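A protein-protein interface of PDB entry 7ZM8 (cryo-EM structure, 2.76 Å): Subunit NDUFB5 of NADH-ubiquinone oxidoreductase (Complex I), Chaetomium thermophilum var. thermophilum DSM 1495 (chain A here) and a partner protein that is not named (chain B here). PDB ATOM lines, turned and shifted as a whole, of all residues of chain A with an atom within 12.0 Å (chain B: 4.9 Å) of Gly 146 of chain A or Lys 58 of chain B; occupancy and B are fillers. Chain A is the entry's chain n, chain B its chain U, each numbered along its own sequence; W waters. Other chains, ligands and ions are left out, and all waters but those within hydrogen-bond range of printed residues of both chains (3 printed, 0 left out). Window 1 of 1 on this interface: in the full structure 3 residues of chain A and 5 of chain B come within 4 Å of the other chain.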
ATOM      1  N   SER A 139     -25.552  10.624  21.313  1.00  0.00           N
ATOM      2  CA  SER A 139     -24.581   9.549  21.418  1.00  0.00           C
ATOM      3  C   SER A 139     -23.537   9.663  20.311  1.00  0.00           C
ATOM      4  O   SER A 139     -23.878   9.925  19.155  1.00  0.00           O
ATOM      5  CB  SER A 139     -25.277   8.193  21.338  1.00  0.00           C
ATOM      6  OG  SER A 139     -24.341   7.133  21.389  1.00  0.00           O
ATOM      7  N   PHE A 141     -21.756   7.077  19.319  1.00  0.00           N
ATOM      8  CA  PHE A 141     -21.484   5.688  18.876  1.00  0.00           C
ATOM      9  C   PHE A 141     -22.586   5.208  17.946  1.00  0.00           C
ATOM     10  O   PHE A 141     -23.729   5.631  18.144  1.00  0.00           O
ATOM     11  CB  PHE A 141     -21.449   4.735  20.070  1.00  0.00           C
ATOM     12  CG  PHE A 141     -20.689   5.253  21.263  1.00  0.00           C
ATOM     13  CD1 PHE A 141     -19.323   5.462  21.195  1.00  0.00           C
ATOM     14  CD2 PHE A 141     -21.341   5.525  22.453  1.00  0.00           C
ATOM     15  CE1 PHE A 141     -18.625   5.940  22.290  1.00  0.00           C
ATOM     16  CE2 PHE A 141     -20.643   6.002  23.548  1.00  0.00           C
ATOM     17  CZ  PHE A 141     -19.288   6.211  23.463  1.00  0.00           C
ATOM     18  N   ASN A 142     -22.233   4.388  16.955  1.00  0.00           N
ATOM     19  CA  ASN A 142     -23.240   3.766  16.058  1.00  0.00           C
ATOM     20  C   ASN A 142     -24.027   4.882  15.398  1.00  0.00           C
ATOM     21  O   ASN A 142     -25.237   4.721  15.208  1.00  0.00           O
ATOM     22  CB  ASN A 142     -24.062   2.704  16.794  1.00  0.00           C
ATOM     23  CG  ASN A 142     -23.206   1.655  17.460  1.00  0.00           C
ATOM     24  OD1 ASN A 142     -22.267   1.146  16.857  1.00  0.00           O
ATOM     25  ND2 ASN A 142     -23.521   1.333  18.702  1.00  0.00           N
ATOM     26  N   VAL A 143     -23.334   5.963  15.065  1.00  0.00           N
ATOM     27  CA  VAL A 143     -23.998   7.143  14.455  1.00  0.00           C
ATOM     28  C   VAL A 143     -24.157   6.886  12.956  1.00  0.00           C
ATOM     29  O   VAL A 143     -23.123   6.652  12.310  1.00  0.00           O
ATOM     30  CB  VAL A 143     -23.211   8.433  14.738  1.00  0.00           C
ATOM     31  CG1 VAL A 143     -23.790   9.620  13.986  1.00  0.00           C
ATOM     32  CG2 VAL A 143     -23.121   8.723  16.221  1.00  0.00           C
ATOM     33  N   PRO A 144     -25.379   6.866  12.361  1.00  0.00           N
ATOM     34  CA  PRO A 144     -25.450   6.721  10.919  1.00  0.00           C
ATOM     35  C   PRO A 144     -25.152   8.020  10.161  1.00  0.00           C
ATOM     36  O   PRO A 144     -25.457   9.057  10.666  1.00  0.00           O
ATOM     37  CB  PRO A 144     -26.935   6.432  10.724  1.00  0.00           C
ATOM     38  CG  PRO A 144     -27.498   6.136  12.096  1.00  0.00           C
ATOM     39  CD  PRO A 144     -26.666   6.972  13.033  1.00  0.00           C
ATOM     40  N   ALA A 145     -24.485   7.949   9.015  1.00  0.00           N
ATOM     41  CA  ALA A 145     -24.136   9.152   8.223  1.00  0.00           C
ATOM     42  C   ALA A 145     -25.391   9.961   7.883  1.00  0.00           C
ATOM     43  O   ALA A 145     -26.395   9.356   7.453  1.00  0.00           O
ATOM     44  CB  ALA A 145     -23.364   8.777   6.992  1.00  0.00           C
ATOM     45  N   GLY A 146     -25.332  11.275   8.074  1.00  0.00           N
ATOM     46  CA  GLY A 146     -26.476  12.140   7.771  1.00  0.00           C
ATOM     47  C   GLY A 146     -27.518  12.123   8.859  1.00  0.00           C
ATOM     48  O   GLY A 146     -28.592  12.706   8.644  1.00  0.00           O
ATOM     49  N   PHE A 147     -27.258  11.444   9.971  1.00  0.00           N
ATOM     50  CA  PHE A 147     -28.221  11.484  11.095  1.00  0.00           C
ATOM     51  C   PHE A 147     -28.242  12.860  11.746  1.00  0.00           C
ATOM     52  O   PHE A 147     -29.326  13.433  11.867  1.00  0.00           O
ATOM     53  CB  PHE A 147     -27.910  10.381  12.109  1.00  0.00           C
ATOM     54  CG  PHE A 147     -28.745  10.403  13.359  1.00  0.00           C
ATOM     55  CD1 PHE A 147     -28.389  11.200  14.432  1.00  0.00           C
ATOM     56  CD2 PHE A 147     -29.877   9.618  13.461  1.00  0.00           C
ATOM     57  CE1 PHE A 147     -29.161  11.229  15.576  1.00  0.00           C
ATOM     58  CE2 PHE A 147     -30.639   9.632  14.614  1.00  0.00           C
ATOM     59  CZ  PHE A 147     -30.274  10.435  15.666  1.00  0.00           C
ATOM     60  N   TYR A 148     -27.080  13.403  12.081  1.00  0.00           N
ATOM     61  CA  TYR A 148     -27.063  14.669  12.853  1.00  0.00           C
ATOM     62  C   TYR A 148     -27.205  15.881  11.947  1.00  0.00           C
ATOM     63  O   TYR A 148     -26.495  15.980  10.951  1.00  0.00           O
ATOM     64  CB  TYR A 148     -25.814  14.801  13.711  1.00  0.00           C
ATOM     65  CG  TYR A 148     -25.809  14.001  14.983  1.00  0.00           C
ATOM     66  CD1 TYR A 148     -26.537  14.408  16.085  1.00  0.00           C
ATOM     67  CD2 TYR A 148     -25.049  12.853  15.091  1.00  0.00           C
ATOM     68  CE1 TYR A 148     -26.516  13.683  17.262  1.00  0.00           C
ATOM     69  CE2 TYR A 148     -25.022  12.113  16.257  1.00  0.00           C
ATOM     70  CZ  TYR A 148     -25.759  12.532  17.345  1.00  0.00           C
ATOM     71  OH  TYR A 148     -25.744  11.798  18.486  1.00  0.00           O
ATOM     72  N   PRO A 149     -28.104  16.821  12.289  1.00  0.00           N
ATOM     73  CA  PRO A 149     -28.334  17.992  11.466  1.00  0.00           C
ATOM     74  C   PRO A 149     -27.190  18.996  11.546  1.00  0.00           C
ATOM     75  O   PRO A 149     -26.456  18.987  12.499  1.00  0.00           O
ATOM     76  CB  PRO A 149     -29.593  18.582  12.098  1.00  0.00           C
ATOM     77  CG  PRO A 149     -29.538  18.152  13.538  1.00  0.00           C
ATOM     78  CD  PRO A 149     -28.964  16.757  13.474  1.00  0.00           C
ATOM     79  N   ASN A 150     -27.065  19.819  10.522  1.00  0.00           N
ATOM     80  CA  ASN A 150     -26.024  20.836  10.507  1.00  0.00           C
ATOM     81  C   ASN A 150     -26.472  22.019  11.355  1.00  0.00           C
ATOM     82  O   ASN A 150     -27.535  22.597  11.109  1.00  0.00           O
ATOM     83  CB  ASN A 150     -25.729  21.262   9.071  1.00  0.00           C
ATOM     84  CG  ASN A 150     -24.656  22.320   8.985  1.00  0.00           C
ATOM     85  OD1 ASN A 150     -24.940  23.481   8.707  1.00  0.00           O
ATOM     86  ND2 ASN A 150     -23.416  21.929   9.241  1.00  0.00           N
ATOM     87  N   LEU A 151     -25.672  22.374  12.356  1.00  0.00           N
ATOM     88  CA  LEU A 151     -26.029  23.392  13.331  1.00  0.00           C
ATOM     89  C   LEU A 151     -25.010  24.523  13.354  1.00  0.00           C
ATOM     90  O   LEU A 151     -24.790  25.165  14.381  1.00  0.00           O
ATOM     91  CB  LEU A 151     -26.182  22.785  14.723  1.00  0.00           C
ATOM     92  CG  LEU A 151     -27.086  21.563  14.870  1.00  0.00           C
ATOM     93  CD1 LEU A 151     -26.898  20.948  16.238  1.00  0.00           C
ATOM     94  CD2 LEU A 151     -28.537  21.921  14.647  1.00  0.00           C
ATOM     95  N   TYR B  54     -18.494   8.466   0.051  1.00  0.00           N
ATOM     96  CA  TYR B  54     -19.931   8.154   0.190  1.00  0.00           C
ATOM     97  C   TYR B  54     -20.442   8.573   1.561  1.00  0.00           C
ATOM     98  O   TYR B  54     -21.511   9.180   1.641  1.00  0.00           O
ATOM     99  CB  TYR B  54     -20.139   6.680  -0.130  1.00  0.00           C
ATOM    100  CG  TYR B  54     -21.492   6.118   0.197  1.00  0.00           C
ATOM    101  CD1 TYR B  54     -22.590   6.400  -0.593  1.00  0.00           C
ATOM    102  CD2 TYR B  54     -21.656   5.288   1.288  1.00  0.00           C
ATOM    103  CE1 TYR B  54     -23.830   5.870  -0.298  1.00  0.00           C
ATOM    104  CE2 TYR B  54     -22.889   4.751   1.600  1.00  0.00           C
ATOM    105  CZ  TYR B  54     -23.973   5.046   0.802  1.00  0.00           C
ATOM    106  OH  TYR B  54     -25.177   4.508   1.112  1.00  0.00           O
ATOM    107  N   MET B  55     -19.696   8.242   2.599  1.00  0.00           N
ATOM    108  CA  MET B  55     -20.101   8.592   3.981  1.00  0.00           C
ATOM    109  C   MET B  55     -20.072  10.103   4.165  1.00  0.00           C
ATOM    110  O   MET B  55     -21.010  10.626   4.756  1.00  0.00           O
ATOM    111  CB  MET B  55     -19.180   7.874   4.968  1.00  0.00           C
ATOM    112  CG  MET B  55     -19.243   6.369   4.814  1.00  0.00           C
ATOM    113  SD  MET B  55     -20.884   5.683   5.126  1.00  0.00           S
ATOM    114  CE  MET B  55     -21.011   5.934   6.895  1.00  0.00           C
ATOM    115  N   GLN B  56     -19.052  10.771   3.629  1.00  0.00           N
ATOM    116  CA  GLN B  56     -18.925  12.243   3.708  1.00  0.00           C
ATOM    117  C   GLN B  56     -20.089  12.914   2.975  1.00  0.00           C
ATOM    118  O   GLN B  56     -20.619  13.871   3.517  1.00  0.00           O
ATOM    119  CB  GLN B  56     -17.570  12.662   3.151  1.00  0.00           C
ATOM    120  CG  GLN B  56     -16.574  13.111   4.201  1.00  0.00           C
ATOM    121  CD  GLN B  56     -15.276  13.463   3.524  1.00  0.00           C
ATOM    122  OE1 GLN B  56     -14.993  13.000   2.423  1.00  0.00           O
ATOM    123  NE2 GLN B  56     -14.477  14.289   4.178  1.00  0.00           N
ATOM    124  N   CYS B  57     -20.488  12.405   1.805  1.00  0.00           N
ATOM    125  CA  CYS B  57     -21.642  12.901   0.994  1.00  0.00           C
ATOM    126  C   CYS B  57     -22.937  12.837   1.761  1.00  0.00           C
ATOM    127  O   CYS B  57     -23.707  13.784   1.660  1.00  0.00           O
ATOM    128  CB  CYS B  57     -21.903  11.972  -0.186  1.00  0.00           C
ATOM    129  SG  CYS B  57     -23.288  12.407  -1.280  1.00  0.00           S
ATOM    130  N   LYS B  58     -23.258  11.677   2.329  1.00  0.00           N
ATOM    131  CA  LYS B  58     -24.533  11.496   3.068  1.00  0.00           C
ATOM    132  C   LYS B  58     -24.551  12.431   4.264  1.00  0.00           C
ATOM    133  O   LYS B  58     -25.638  12.827   4.667  1.00  0.00           O
ATOM    134  CB  LYS B  58     -24.615  10.064   3.594  1.00  0.00           C
ATOM    135  CG  LYS B  58     -24.771   8.978   2.542  1.00  0.00           C
ATOM    136  CD  LYS B  58     -25.491   7.769   3.075  1.00  0.00           C
ATOM    137  CE  LYS B  58     -26.854   8.108   3.637  1.00  0.00           C
ATOM    138  NZ  LYS B  58     -27.712   6.907   3.763  1.00  0.00           N
ATOM    139  N   ASN B  59     -23.386  12.673   4.850  1.00  0.00           N
ATOM    140  CA  ASN B  59     -23.248  13.570   6.015  1.00  0.00           C
ATOM    141  C   ASN B  59     -23.554  14.989   5.565  1.00  0.00           C
ATOM    142  O   ASN B  59     -24.137  15.741   6.355  1.00  0.00           O
ATOM    143  CB  ASN B  59     -21.855  13.452   6.619  1.00  0.00           C
ATOM    144  CG  ASN B  59     -21.827  12.799   7.983  1.00  0.00           C
ATOM    145  OD1 ASN B  59     -22.839  12.309   8.466  1.00  0.00           O
ATOM    146  ND2 ASN B  59     -20.666  12.798   8.615  1.00  0.00           N
ATOM    147  N   GLU B  60     -23.130  15.346   4.358  1.00  0.00           N
ATOM    148  CA  GLU B  60     -23.331  16.714   3.826  1.00  0.00           C
ATOM    149  C   GLU B  60     -24.806  16.922   3.479  1.00  0.00           C
ATOM    150  O   GLU B  60     -25.202  18.082   3.278  1.00  0.00           O
ATOM    151  CB  GLU B  60     -22.442  16.938   2.608  1.00  0.00           C
ATOM    152  CG  GLU B  60     -20.988  17.175   2.958  1.00  0.00           C
ATOM    153  CD  GLU B  60     -20.188  17.823   1.845  1.00  0.00           C
ATOM    154  OE1 GLU B  60     -20.704  17.894   0.712  1.00  0.00           O
ATOM    155  OE2 GLU B  60     -19.054  18.266   2.114  1.00  0.00           O
ATOM    156  N   ASN B  61     -25.597  15.855   3.424  1.00  0.00           N
ATOM    157  CA  ASN B  61     -27.049  16.020   3.197  1.00  0.00           C
ATOM    158  C   ASN B  61     -27.816  15.282   4.287  1.00  0.00           C
ATOM    159  O   ASN B  61     -28.255  14.157   4.051  1.00  0.00           O
ATOM    160  CB  ASN B  61     -27.426  15.417   1.846  1.00  0.00           C
ATOM    161  CG  ASN B  61     -26.658  16.017   0.691  1.00  0.00           C
ATOM    162  OD1 ASN B  61     -26.911  17.151   0.294  1.00  0.00           O
ATOM    163  ND2 ASN B  61     -25.722  15.263   0.140  1.00  0.00           N
ATOM    164  N   PRO B  62     -28.076  15.936   5.436  1.00  0.00           N
ATOM    165  CA  PRO B  62     -28.806  15.304   6.536  1.00  0.00           C
ATOM    166  C   PRO B  62     -30.303  15.070   6.262  1.00  0.00           C
ATOM    167  O   PRO B  62     -30.985  16.009   5.936  1.00  0.00           O
ATOM    168  CB  PRO B  62     -28.556  16.278   7.706  1.00  0.00           C
ATOM    169  CG  PRO B  62     -27.396  17.130   7.259  1.00  0.00           C
ATOM    170  CD  PRO B  62     -27.613  17.277   5.772  1.00  0.00           C
ATOM    171  N   GLY B  63     -30.769  13.836   6.415  1.00  0.00           N
ATOM    172  CA  GLY B  63     -32.184  13.472   6.198  1.00  0.00           C
ATOM    173  C   GLY B  63     -32.497  13.250   4.737  1.00  0.00           C
ATOM    174  O   GLY B  63     -33.623  12.876   4.441  1.00  0.00           O
ATOM    175  N   GLY B  65     -29.944  11.804   2.440  1.00  0.00           N
ATOM    176  CA  GLY B  65     -28.744  11.162   1.880  1.00  0.00           C
ATOM    177  C   GLY B  65     -28.988   9.848   1.194  1.00  0.00           C
ATOM    178  O   GLY B  65     -28.117   9.467   0.412  1.00  0.00           O
ATOM    179  N   GLU B  66     -30.090   9.153   1.473  1.00  0.00           N
ATOM    180  CA  GLU B  66     -30.360   7.917   0.696  1.00  0.00           C
ATOM    181  C   GLU B  66     -30.521   8.340  -0.757  1.00  0.00           C
ATOM    182  O   GLU B  66     -29.894   7.726  -1.607  1.00  0.00           O
ATOM    183  CB  GLU B  66     -31.608   7.273   1.293  1.00  0.00           C
ATOM    184  CG  GLU B  66     -31.410   6.742   2.702  1.00  0.00           C
ATOM    185  CD  GLU B  66     -31.352   7.754   3.838  1.00  0.00           C
ATOM    186  OE1 GLU B  66     -31.884   8.873   3.676  1.00  0.00           O
ATOM    187  OE2 GLU B  66     -30.765   7.420   4.887  1.00  0.00           O
ATOM    188  N   CYS B  69     -27.296  10.766  -2.759  1.00  0.00           N
ATOM    189  CA  CYS B  69     -25.938  10.149  -2.673  1.00  0.00           C
ATOM    190  C   CYS B  69     -25.938   8.816  -3.432  1.00  0.00           C
ATOM    191  O   CYS B  69     -25.094   7.977  -3.129  1.00  0.00           O
ATOM    192  CB  CYS B  69     -25.395  10.065  -1.247  1.00  0.00           C
ATOM    193  SG  CYS B  69     -25.044  11.676  -0.490  1.00  0.00           S
HETATM  194  O   HOH W   1     -24.808  14.893   9.125  1.00  0.00           O
HETATM  195  O   HOH W   2     -30.042  11.010   7.005  1.00  0.00           O
HETATM  196  O   HOH W   3     -24.229  12.306  11.545  1.00  0.00           O
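The backbone NH of Gly 63 of chain B sits at hydrogen-bond distance from the backbone carbonyl oxygen of Gly 146 of chain A.
The backbone NH (N) of Gly 146 of chain A sits at hydrogen-bond distance from the side-chain amide oxygen (OD1) of Asn 59 of chain B (2.7 Å).
Water W1 lies within hydrogen-bond range of the backbone carbonyl oxygen of Tyr 148 of chain A and the backbone carbonyl oxygen of Asn 59 of chain B.
Water W2 lies within hydrogen-bond range of O of Gly 146 of chain A (2.8 Å) and N of Gly 63 of chain B (3.0 Å).
Water W3 lies within hydrogen-bond range of N of Tyr 148 of chain A and OD1 of Asn 59 of chain B.
Printed residues of chain B that touch a printed residue of chain A: Met 55, Lys 58, Asn 59, Pro 62 and Gly 63.
Hydrophobic or aromatic side chains of chain B that line the printed part of chain A: Met 55 and Pro 62.
Along chain B the printed residues that touch a printed residue of chain A span positions 55 to 63.
Among the printed residues, no Asp or Glu carboxylate lies within 4 Å of a Lys or Arg side-chain nitrogen of the other chain.
Among the printed residues, merely in contact across the chains: Ala 145 of chain A with Met 55 of chain B, Ala 145 of chain A with Lys 58 of chain B, Ala 145 of chain A with Asn 59 of chain B, Gly 146 of chain A with Lys 58 of chain B, Gly 146 of chain A with Pro 62 of chain B and Tyr 148 of chain A with Pro 62 of chain B.
Of the printed residues of chain B, Ala 145 of chain A touches Met 55 (3.7 Å), Lys 58 (3.8 Å) and Asn 59 (3.4 Å).
Of chain B, only Lys 58, Asn 59, Pro 62 and Gly 63 come within 4 Å of Gly 146 of chain A.
Printed residues of chain B within 4 Å of Tyr 148 of chain A: Pro 62 (3.9 Å).
Met 55 of chain B touches just one residue of chain A: Ala 145 (3.7 Å).
Of chain A, only Ala 145 and Gly 146 come within 4 Å of Lys 58 of chain B.
Of chain A, only Gly 146 (3.4 Å) and Tyr 148 (3.9 Å) come within 4 Å of Pro 62 of chain B.
Gly 63 of chain B touches just one residue of chain A: Gly 146.
No residue of chain A comes within 4 Å of Gly 65 of chain B.
No residue of chain A comes within 4 Å of Glu 66 of chain B.
The nearest residue of chain B that does not touch Gly 146 of chain A is Asn 61 of chain B (4.6 Å).
The nearest printed residue of chain B that does not touch Ala 145 of chain A is Glu 66 of chain B (5.4 Å).
SG of Cys 57 of chain B forms a disulfide with SG of Cys 69 of chain B, 2.1 Å away.
The side-chain amino group (NZ) of Lys 58 of chain B is in salt-bridge range of the side-chain carboxylate (OE2) of Glu 66 of chain B (3.3 Å).
O of Ser 139 of chain A is in hydrogen-bond range of OH of Tyr 148 of chain A (2.7 Å).
N of Lys 58 of chain B is in hydrogen-bond range of SG of Cys 69 of chain B.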
